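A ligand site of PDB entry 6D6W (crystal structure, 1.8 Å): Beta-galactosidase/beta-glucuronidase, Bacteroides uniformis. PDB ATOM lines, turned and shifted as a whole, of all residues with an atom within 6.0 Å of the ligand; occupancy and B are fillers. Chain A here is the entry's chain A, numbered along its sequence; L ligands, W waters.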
ATOM      1  N   ASP A 189     -21.472  -5.572  12.442  1.00  0.00           N
ATOM      2  CA  ASP A 189     -22.383  -6.701  12.222  1.00  0.00           C
ATOM      3  C   ASP A 189     -21.699  -8.041  12.411  1.00  0.00           C
ATOM      4  O   ASP A 189     -21.960  -8.976  11.642  1.00  0.00           O
ATOM      5  CB  ASP A 189     -23.057  -6.619  10.848  1.00  0.00           C
ATOM      6  CG  ASP A 189     -24.242  -7.588  10.713  1.00  0.00           C
ATOM      7  OD1 ASP A 189     -25.081  -7.682  11.673  1.00  0.00           O
ATOM      8  OD2 ASP A 189     -24.374  -8.227   9.647  1.00  0.00           O
ATOM      9  N   TRP A 190     -20.829  -8.179  13.413  1.00  0.00           N
ATOM     10  CA  TRP A 190     -20.280  -9.486  13.737  1.00  0.00           C
ATOM     11  C   TRP A 190     -20.063  -9.551  15.244  1.00  0.00           C
ATOM     12  O   TRP A 190     -20.076  -8.527  15.936  1.00  0.00           O
ATOM     13  CB  TRP A 190     -18.979  -9.781  12.976  1.00  0.00           C
ATOM     14  CG  TRP A 190     -17.784  -8.960  13.392  1.00  0.00           C
ATOM     15  CD1 TRP A 190     -16.940  -9.199  14.455  1.00  0.00           C
ATOM     16  CD2 TRP A 190     -17.273  -7.789  12.739  1.00  0.00           C
ATOM     17  NE1 TRP A 190     -15.955  -8.236  14.503  1.00  0.00           N
ATOM     18  CE2 TRP A 190     -16.123  -7.368  13.462  1.00  0.00           C
ATOM     19  CE3 TRP A 190     -17.662  -7.047  11.608  1.00  0.00           C
ATOM     20  CZ2 TRP A 190     -15.379  -6.239  13.103  1.00  0.00           C
ATOM     21  CZ3 TRP A 190     -16.907  -5.931  11.247  1.00  0.00           C
ATOM     22  CH2 TRP A 190     -15.787  -5.543  11.986  1.00  0.00           C
ATOM     23  N   HIS A 322     -15.840 -14.582   6.857  1.00  0.00           N
ATOM     24  CA  HIS A 322     -15.427 -14.127   8.178  1.00  0.00           C
ATOM     25  C   HIS A 322     -14.463 -15.141   8.788  1.00  0.00           C
ATOM     26  O   HIS A 322     -14.455 -16.315   8.417  1.00  0.00           O
ATOM     27  CB  HIS A 322     -16.619 -13.936   9.124  1.00  0.00           C
ATOM     28  CG  HIS A 322     -17.056 -12.513   9.262  1.00  0.00           C
ATOM     29  ND1 HIS A 322     -16.303 -11.553   9.895  1.00  0.00           N
ATOM     30  CD2 HIS A 322     -18.178 -11.884   8.822  1.00  0.00           C
ATOM     31  CE1 HIS A 322     -16.931 -10.400   9.857  1.00  0.00           C
ATOM     32  NE2 HIS A 322     -18.078 -10.570   9.221  1.00  0.00           N
ATOM     33  N   ARG A 354     -12.545 -12.878  -0.365  1.00  0.00           N
ATOM     34  CA  ARG A 354     -12.441 -11.630   0.384  1.00  0.00           C
ATOM     35  C   ARG A 354     -12.471 -11.994   1.859  1.00  0.00           C
ATOM     36  O   ARG A 354     -13.468 -12.526   2.348  1.00  0.00           O
ATOM     37  CB  ARG A 354     -13.595 -10.677   0.049  1.00  0.00           C
ATOM     38  CG  ARG A 354     -13.633  -9.437   0.930  1.00  0.00           C
ATOM     39  CD  ARG A 354     -14.893  -8.605   0.733  1.00  0.00           C
ATOM     40  NE  ARG A 354     -14.826  -7.374   1.512  1.00  0.00           N
ATOM     41  CZ  ARG A 354     -15.883  -6.767   2.045  1.00  0.00           C
ATOM     42  NH1 ARG A 354     -17.085  -7.293   1.904  1.00  0.00           N
ATOM     43  NH2 ARG A 354     -15.716  -5.656   2.751  1.00  0.00           N
ATOM     44  N   HIS A 357     -13.628  -8.772   8.249  1.00  0.00           N
ATOM     45  CA  HIS A 357     -13.476  -7.349   7.906  1.00  0.00           C
ATOM     46  C   HIS A 357     -12.213  -6.790   8.575  1.00  0.00           C
ATOM     47  O   HIS A 357     -12.188  -5.640   8.999  1.00  0.00           O
ATOM     48  CB  HIS A 357     -14.672  -6.538   8.414  1.00  0.00           C
ATOM     49  CG  HIS A 357     -15.903  -6.626   7.566  1.00  0.00           C
ATOM     50  ND1 HIS A 357     -15.967  -6.107   6.291  1.00  0.00           N
ATOM     51  CD2 HIS A 357     -17.137  -7.119   7.821  1.00  0.00           C
ATOM     52  CE1 HIS A 357     -17.178  -6.285   5.800  1.00  0.00           C
ATOM     53  NE2 HIS A 357     -17.918  -6.892   6.716  1.00  0.00           N
ATOM     54  N   TYR A 382     -14.619   0.525   9.821  1.00  0.00           N
ATOM     55  CA  TYR A 382     -15.908  -0.053   9.469  1.00  0.00           C
ATOM     56  C   TYR A 382     -17.014   0.796  10.072  1.00  0.00           C
ATOM     57  O   TYR A 382     -16.997   1.056  11.285  1.00  0.00           O
ATOM     58  CB  TYR A 382     -15.935  -1.504   9.961  1.00  0.00           C
ATOM     59  CG  TYR A 382     -17.189  -2.324   9.775  1.00  0.00           C
ATOM     60  CD1 TYR A 382     -17.281  -3.261   8.761  1.00  0.00           C
ATOM     61  CD2 TYR A 382     -18.262  -2.194  10.656  1.00  0.00           C
ATOM     62  CE1 TYR A 382     -18.436  -4.052   8.617  1.00  0.00           C
ATOM     63  CE2 TYR A 382     -19.419  -2.964  10.505  1.00  0.00           C
ATOM     64  CZ  TYR A 382     -19.492  -3.895   9.500  1.00  0.00           C
ATOM     65  OH  TYR A 382     -20.638  -4.662   9.404  1.00  0.00           O
ATOM     66  N   TRP A 383     -17.923   1.276   9.225  1.00  0.00           N
ATOM     67  CA  TRP A 383     -19.067   2.124   9.633  1.00  0.00           C
ATOM     68  C   TRP A 383     -18.574   3.412  10.311  1.00  0.00           C
ATOM     69  O   TRP A 383     -17.726   4.110   9.728  1.00  0.00           O
ATOM     70  CB  TRP A 383     -20.020   1.285  10.470  1.00  0.00           C
ATOM     71  CG  TRP A 383     -20.763   0.233   9.688  1.00  0.00           C
ATOM     72  CD1 TRP A 383     -20.641  -0.060   8.353  1.00  0.00           C
ATOM     73  CD2 TRP A 383     -21.755  -0.652  10.210  1.00  0.00           C
ATOM     74  NE1 TRP A 383     -21.482  -1.106   8.018  1.00  0.00           N
ATOM     75  CE2 TRP A 383     -22.185  -1.480   9.145  1.00  0.00           C
ATOM     76  CE3 TRP A 383     -22.313  -0.840  11.483  1.00  0.00           C
ATOM     77  CZ2 TRP A 383     -23.152  -2.475   9.313  1.00  0.00           C
ATOM     78  CZ3 TRP A 383     -23.280  -1.836  11.651  1.00  0.00           C
ATOM     79  CH2 TRP A 383     -23.678  -2.643  10.565  1.00  0.00           C
ATOM     80  N   ASN A 420     -14.822  -0.097   5.018  1.00  0.00           N
ATOM     81  CA  ASN A 420     -16.061  -0.757   4.624  1.00  0.00           C
ATOM     82  C   ASN A 420     -17.271   0.054   5.099  1.00  0.00           C
ATOM     83  O   ASN A 420     -17.463   0.226   6.303  1.00  0.00           O
ATOM     84  CB  ASN A 420     -16.097  -2.199   5.168  1.00  0.00           C
ATOM     85  CG  ASN A 420     -17.373  -2.950   4.802  1.00  0.00           C
ATOM     86  OD1 ASN A 420     -17.444  -3.603   3.767  1.00  0.00           O
ATOM     87  ND2 ASN A 420     -18.390  -2.839   5.651  1.00  0.00           N
ATOM     88  N   GLU A 421     -18.048   0.568   4.143  1.00  0.00           N
ATOM     89  CA  GLU A 421     -19.345   1.202   4.407  1.00  0.00           C
ATOM     90  C   GLU A 421     -19.242   2.372   5.384  1.00  0.00           C
ATOM     91  O   GLU A 421     -19.946   2.436   6.407  1.00  0.00           O
ATOM     92  CB  GLU A 421     -20.363   0.163   4.885  1.00  0.00           C
ATOM     93  CG  GLU A 421     -20.729  -0.803   3.778  1.00  0.00           C
ATOM     94  CD  GLU A 421     -22.047  -1.492   4.026  1.00  0.00           C
ATOM     95  OE1 GLU A 421     -22.529  -1.475   5.178  1.00  0.00           O
ATOM     96  OE2 GLU A 421     -22.597  -2.026   3.043  1.00  0.00           O
ATOM     97  N   ASN A 478     -20.516  -2.469  -2.004  1.00  0.00           N
ATOM     98  CA  ASN A 478     -21.525  -3.411  -1.563  1.00  0.00           C
ATOM     99  C   ASN A 478     -22.880  -2.989  -2.100  1.00  0.00           C
ATOM    100  O   ASN A 478     -23.210  -1.799  -2.095  1.00  0.00           O
ATOM    101  CB  ASN A 478     -21.618  -3.448  -0.027  1.00  0.00           C
ATOM    102  CG  ASN A 478     -20.333  -3.908   0.636  1.00  0.00           C
ATOM    103  OD1 ASN A 478     -19.415  -4.398  -0.018  1.00  0.00           O
ATOM    104  ND2 ASN A 478     -20.285  -3.790   1.959  1.00  0.00           N
ATOM    105  N   TYR A 480     -27.147  -4.512  -2.190  1.00  0.00           N
ATOM    106  CA  TYR A 480     -28.100  -5.534  -1.763  1.00  0.00           C
ATOM    107  C   TYR A 480     -29.435  -5.357  -2.472  1.00  0.00           C
ATOM    108  O   TYR A 480     -30.495  -5.460  -1.856  1.00  0.00           O
ATOM    109  CB  TYR A 480     -28.289  -5.504  -0.247  1.00  0.00           C
ATOM    110  CG  TYR A 480     -27.149  -6.192   0.453  1.00  0.00           C
ATOM    111  CD1 TYR A 480     -26.058  -5.472   0.918  1.00  0.00           C
ATOM    112  CD2 TYR A 480     -27.123  -7.571   0.604  1.00  0.00           C
ATOM    113  CE1 TYR A 480     -24.991  -6.097   1.529  1.00  0.00           C
ATOM    114  CE2 TYR A 480     -26.062  -8.215   1.216  1.00  0.00           C
ATOM    115  CZ  TYR A 480     -24.995  -7.469   1.671  1.00  0.00           C
ATOM    116  OH  TYR A 480     -23.923  -8.096   2.273  1.00  0.00           O
ATOM    117  N   TYR A 484     -32.128  -6.004   0.877  1.00  0.00           N
ATOM    118  CA  TYR A 484     -32.439  -4.768   1.599  1.00  0.00           C
ATOM    119  C   TYR A 484     -33.127  -3.737   0.719  1.00  0.00           C
ATOM    120  O   TYR A 484     -33.906  -2.908   1.216  1.00  0.00           O
ATOM    121  CB  TYR A 484     -31.161  -4.150   2.175  1.00  0.00           C
ATOM    122  CG  TYR A 484     -30.513  -4.958   3.269  1.00  0.00           C
ATOM    123  CD1 TYR A 484     -31.241  -5.378   4.382  1.00  0.00           C
ATOM    124  CD2 TYR A 484     -29.163  -5.279   3.215  1.00  0.00           C
ATOM    125  CE1 TYR A 484     -30.634  -6.108   5.415  1.00  0.00           C
ATOM    126  CE2 TYR A 484     -28.545  -6.014   4.232  1.00  0.00           C
ATOM    127  CZ  TYR A 484     -29.284  -6.412   5.332  1.00  0.00           C
ATOM    128  OH  TYR A 484     -28.683  -7.143   6.337  1.00  0.00           O
ATOM    129  N   GLU A 508     -19.834  -7.128  -1.884  1.00  0.00           N
ATOM    130  CA  GLU A 508     -20.890  -7.815  -1.157  1.00  0.00           C
ATOM    131  C   GLU A 508     -22.160  -7.731  -1.969  1.00  0.00           C
ATOM    132  O   GLU A 508     -22.424  -6.709  -2.628  1.00  0.00           O
ATOM    133  CB  GLU A 508     -21.147  -7.237   0.242  1.00  0.00           C
ATOM    134  CG  GLU A 508     -20.057  -7.495   1.283  1.00  0.00           C
ATOM    135  CD  GLU A 508     -20.402  -6.956   2.674  1.00  0.00           C
ATOM    136  OE1 GLU A 508     -19.480  -6.484   3.385  1.00  0.00           O
ATOM    137  OE2 GLU A 508     -21.587  -7.019   3.054  1.00  0.00           O
ATOM    138  N   TRP A 553     -21.728 -11.986  -0.225  1.00  0.00           N
ATOM    139  CA  TRP A 553     -21.843 -12.099   1.232  1.00  0.00           C
ATOM    140  C   TRP A 553     -22.899 -13.174   1.489  1.00  0.00           C
ATOM    141  O   TRP A 553     -24.094 -12.912   1.317  1.00  0.00           O
ATOM    142  CB  TRP A 553     -22.277 -10.743   1.793  1.00  0.00           C
ATOM    143  CG  TRP A 553     -22.066 -10.572   3.252  1.00  0.00           C
ATOM    144  CD1 TRP A 553     -23.017 -10.570   4.223  1.00  0.00           C
ATOM    145  CD2 TRP A 553     -20.815 -10.378   3.886  1.00  0.00           C
ATOM    146  NE1 TRP A 553     -22.414 -10.376   5.459  1.00  0.00           N
ATOM    147  CE2 TRP A 553     -21.059 -10.245   5.263  1.00  0.00           C
ATOM    148  CE3 TRP A 553     -19.495 -10.280   3.410  1.00  0.00           C
ATOM    149  CZ2 TRP A 553     -20.035 -10.039   6.177  1.00  0.00           C
ATOM    150  CZ3 TRP A 553     -18.480 -10.072   4.318  1.00  0.00           C
ATOM    151  CH2 TRP A 553     -18.762  -9.961   5.691  1.00  0.00           C
ATOM    152  N   PHE A 558     -22.672 -16.662   9.940  1.00  0.00           N
ATOM    153  CA  PHE A 558     -21.778 -16.284  11.038  1.00  0.00           C
ATOM    154  C   PHE A 558     -22.537 -15.567  12.153  1.00  0.00           C
ATOM    155  O   PHE A 558     -23.688 -15.139  11.984  1.00  0.00           O
ATOM    156  CB  PHE A 558     -20.628 -15.410  10.534  1.00  0.00           C
ATOM    157  CG  PHE A 558     -21.073 -14.127   9.892  1.00  0.00           C
ATOM    158  CD1 PHE A 558     -21.524 -14.099   8.589  1.00  0.00           C
ATOM    159  CD2 PHE A 558     -21.045 -12.943  10.624  1.00  0.00           C
ATOM    160  CE1 PHE A 558     -21.952 -12.897   8.006  1.00  0.00           C
ATOM    161  CE2 PHE A 558     -21.475 -11.760  10.056  1.00  0.00           C
ATOM    162  CZ  PHE A 558     -21.913 -11.727   8.736  1.00  0.00           C
ATOM    163  N   ARG A 562     -26.948  -8.526  15.855  1.00  0.00           N
ATOM    164  CA  ARG A 562     -27.966  -7.699  15.216  1.00  0.00           C
ATOM    165  C   ARG A 562     -28.950  -8.531  14.401  1.00  0.00           C
ATOM    166  O   ARG A 562     -29.629  -7.993  13.524  1.00  0.00           O
ATOM    167  CB  ARG A 562     -27.297  -6.642  14.319  1.00  0.00           C
ATOM    168  CG  ARG A 562     -26.230  -5.822  15.045  1.00  0.00           C
ATOM    169  CD  ARG A 562     -25.487  -4.886  14.095  1.00  0.00           C
ATOM    170  NE  ARG A 562     -26.342  -3.864  13.454  1.00  0.00           N
ATOM    171  CZ  ARG A 562     -26.739  -3.900  12.179  1.00  0.00           C
ATOM    172  NH1 ARG A 562     -26.413  -4.918  11.391  1.00  0.00           N
ATOM    173  NH2 ARG A 562     -27.486  -2.900  11.697  1.00  0.00           N
ATOM    174  N   ARG A 563     -29.052  -9.827  14.690  1.00  0.00           N
ATOM    175  CA  ARG A 563     -29.861 -10.738  13.885  1.00  0.00           C
ATOM    176  C   ARG A 563     -30.775 -11.535  14.820  1.00  0.00           C
ATOM    177  O   ARG A 563     -30.355 -12.536  15.401  1.00  0.00           O
ATOM    178  CB  ARG A 563     -28.975 -11.658  13.044  1.00  0.00           C
ATOM    179  CG  ARG A 563     -27.953 -10.895  12.175  1.00  0.00           C
ATOM    180  CD  ARG A 563     -28.636 -10.047  11.072  1.00  0.00           C
ATOM    181  NE  ARG A 563     -27.698  -9.068  10.513  1.00  0.00           N
ATOM    182  CZ  ARG A 563     -27.978  -8.240   9.499  1.00  0.00           C
ATOM    183  NH1 ARG A 563     -29.187  -8.260   8.926  1.00  0.00           N
ATOM    184  NH2 ARG A 563     -27.059  -7.386   9.074  1.00  0.00           N
ATOM    185  N   ASN A 573     -26.167 -14.056  11.288  1.00  0.00           N
ATOM    186  CA  ASN A 573     -26.377 -13.590   9.924  1.00  0.00           C
ATOM    187  C   ASN A 573     -26.540 -14.809   9.020  1.00  0.00           C
ATOM    188  O   ASN A 573     -25.661 -15.685   8.989  1.00  0.00           O
ATOM    189  CB  ASN A 573     -25.178 -12.731   9.504  1.00  0.00           C
ATOM    190  CG  ASN A 573     -25.377 -12.059   8.148  1.00  0.00           C
ATOM    191  OD1 ASN A 573     -25.706 -12.728   7.162  1.00  0.00           O
ATOM    192  ND2 ASN A 573     -25.171 -10.744   8.089  1.00  0.00           N
ATOM    193  N   LYS A 575     -26.830 -15.017   5.697  1.00  0.00           N
ATOM    194  CA  LYS A 575     -26.539 -14.801   4.284  1.00  0.00           C
ATOM    195  C   LYS A 575     -25.537 -15.794   3.719  1.00  0.00           C
ATOM    196  O   LYS A 575     -25.157 -15.669   2.559  1.00  0.00           O
ATOM    197  CB  LYS A 575     -26.088 -13.352   4.085  1.00  0.00           C
ATOM    198  CG  LYS A 575     -27.240 -12.356   4.225  1.00  0.00           C
ATOM    199  CD  LYS A 575     -26.757 -10.915   4.122  1.00  0.00           C
ATOM    200  CE  LYS A 575     -27.842  -9.926   4.538  1.00  0.00           C
ATOM    201  NZ  LYS A 575     -28.084  -9.902   6.058  1.00  0.00           N
HETATM  202  C1  LIG L   1     -22.756  -4.694   5.340  1.00  0.00           C
HETATM  203  C2  LIG L   1     -21.518  -5.194   6.095  1.00  0.00           C
HETATM  204  C3  LIG L   1     -21.620  -6.597   6.549  1.00  0.00           C
HETATM  205  C4  LIG L   1     -22.908  -6.984   7.129  1.00  0.00           C
HETATM  206  C5  LIG L   1     -23.928  -6.809   5.997  1.00  0.00           C
HETATM  207  C6  LIG L   1     -25.337  -7.332   6.284  1.00  0.00           C
HETATM  208  O1  LIG L   1     -22.648  -4.822   3.948  1.00  0.00           O
HETATM  209  O2  LIG L   1     -20.338  -4.931   5.350  1.00  0.00           O
HETATM  210  O3  LIG L   1     -20.578  -6.739   7.479  1.00  0.00           O
HETATM  211  O4  LIG L   1     -22.878  -8.328   7.515  1.00  0.00           O
HETATM  212  O5  LIG L   1     -24.017  -5.395   5.627  1.00  0.00           O
HETATM  213  O6  LIG L   1     -25.537  -8.566   6.250  1.00  0.00           O
HETATM  214  O7  LIG L   1     -26.261  -6.514   6.523  1.00  0.00           O
HETATM  215  O   HOH W   1     -25.189  -2.669   3.047  1.00  0.00           O
HETATM  216  O   HOH W   2     -20.245  -8.583   9.516  1.00  0.00           O
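The side-chain amide nitrogen of Asn 420 is in hydrogen-bond range of an oxygen (O2) of the ligand. The side-chain amide nitrogen (ND2) of Asn 478 sits at hydrogen-bond distance from an oxygen (O1) of the ligand (3.3 Å). The side-chain amino group (NZ) of Lys 575 is in salt-bridge range of an oxygen (O6) of the ligand. An oxygen (O7) of the ligand is in hydrogen-bond range of the side-chain hydroxyl (OH) of Tyr 484. A ring nitrogen (NE2) of His 357 is in hydrogen-bond range of an oxygen (O3) of the ligand, 2.8 Å away. An oxygen (O4) of the ligand is in hydrogen-bond range of the side-chain carboxylate (OD2) of Asp 189, at 2.6 Å. O3 of the ligand sits at hydrogen-bond distance from OH of Tyr 382, 2.8 Å away. O1 of the ligand sits at hydrogen-bond distance from OE2 of Glu 421 (2.9 Å). O1 of the ligand lies within hydrogen-bond range of OE2 of Glu 508 (2.6 Å). NH2 of Arg 563 lies within salt-bridge range of O7 of the ligand (2.8 Å). An oxygen (O6) of the ligand sits at hydrogen-bond distance from the side-chain amide nitrogen (ND2) of Asn 573. NE1 of Trp 553 is in hydrogen-bond range of O4 of the ligand, at 2.9 Å.
The side-chain amide oxygen of Asn 573 is in hydrogen-bond range of the backbone NH of Lys 575, 2.9 Å away. The side-chain carboxylate (OD2) of Asp 189 is in salt-bridge range of the guanidinium group (NH2) of Arg 563. The side-chain amide oxygen (OD1) of Asn 420 is in hydrogen-bond range of the guanidinium group (NH2) of Arg 354 (2.9 Å). NH1 of Arg 354 is in salt-bridge range of OE1 of Glu 508, 2.9 Å away. The side-chain amino group (NZ) of Lys 575 sits at hydrogen-bond distance from the side-chain hydroxyl (OH) of Tyr 484 (2.8 Å). OD1 of Asn 420 sits at hydrogen-bond distance from ND2 of Asn 478, at 3.4 Å. OE1 of Glu 508 is in hydrogen-bond range of ND2 of Asn 478 (3.2 Å). The side-chain carboxylate (OE1) of Glu 421 lies within hydrogen-bond range of the indole nitrogen (NE1) of Trp 383 (3.0 Å).
Tyr 480 touches the ligand (CE1 to O1, 3.6 Å). CZ of Phe 558 touches O4 of the ligand (3.7 Å). Hydrophobic or aromatic side chains within 4 Å of the ligand: His 357, Tyr 382, Tyr 480, Tyr 484, Trp 553 and Phe 558. The nearest printed residue that does not touch the ligand is Trp 383 (4.5 Å).
Water W2 lies within hydrogen-bond range of O of Asp 189, O3 of the ligand and NE2 of His 322. Water W1 bridges the side-chain carboxylate of Glu 421 and an oxygen (O1) of the ligand.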
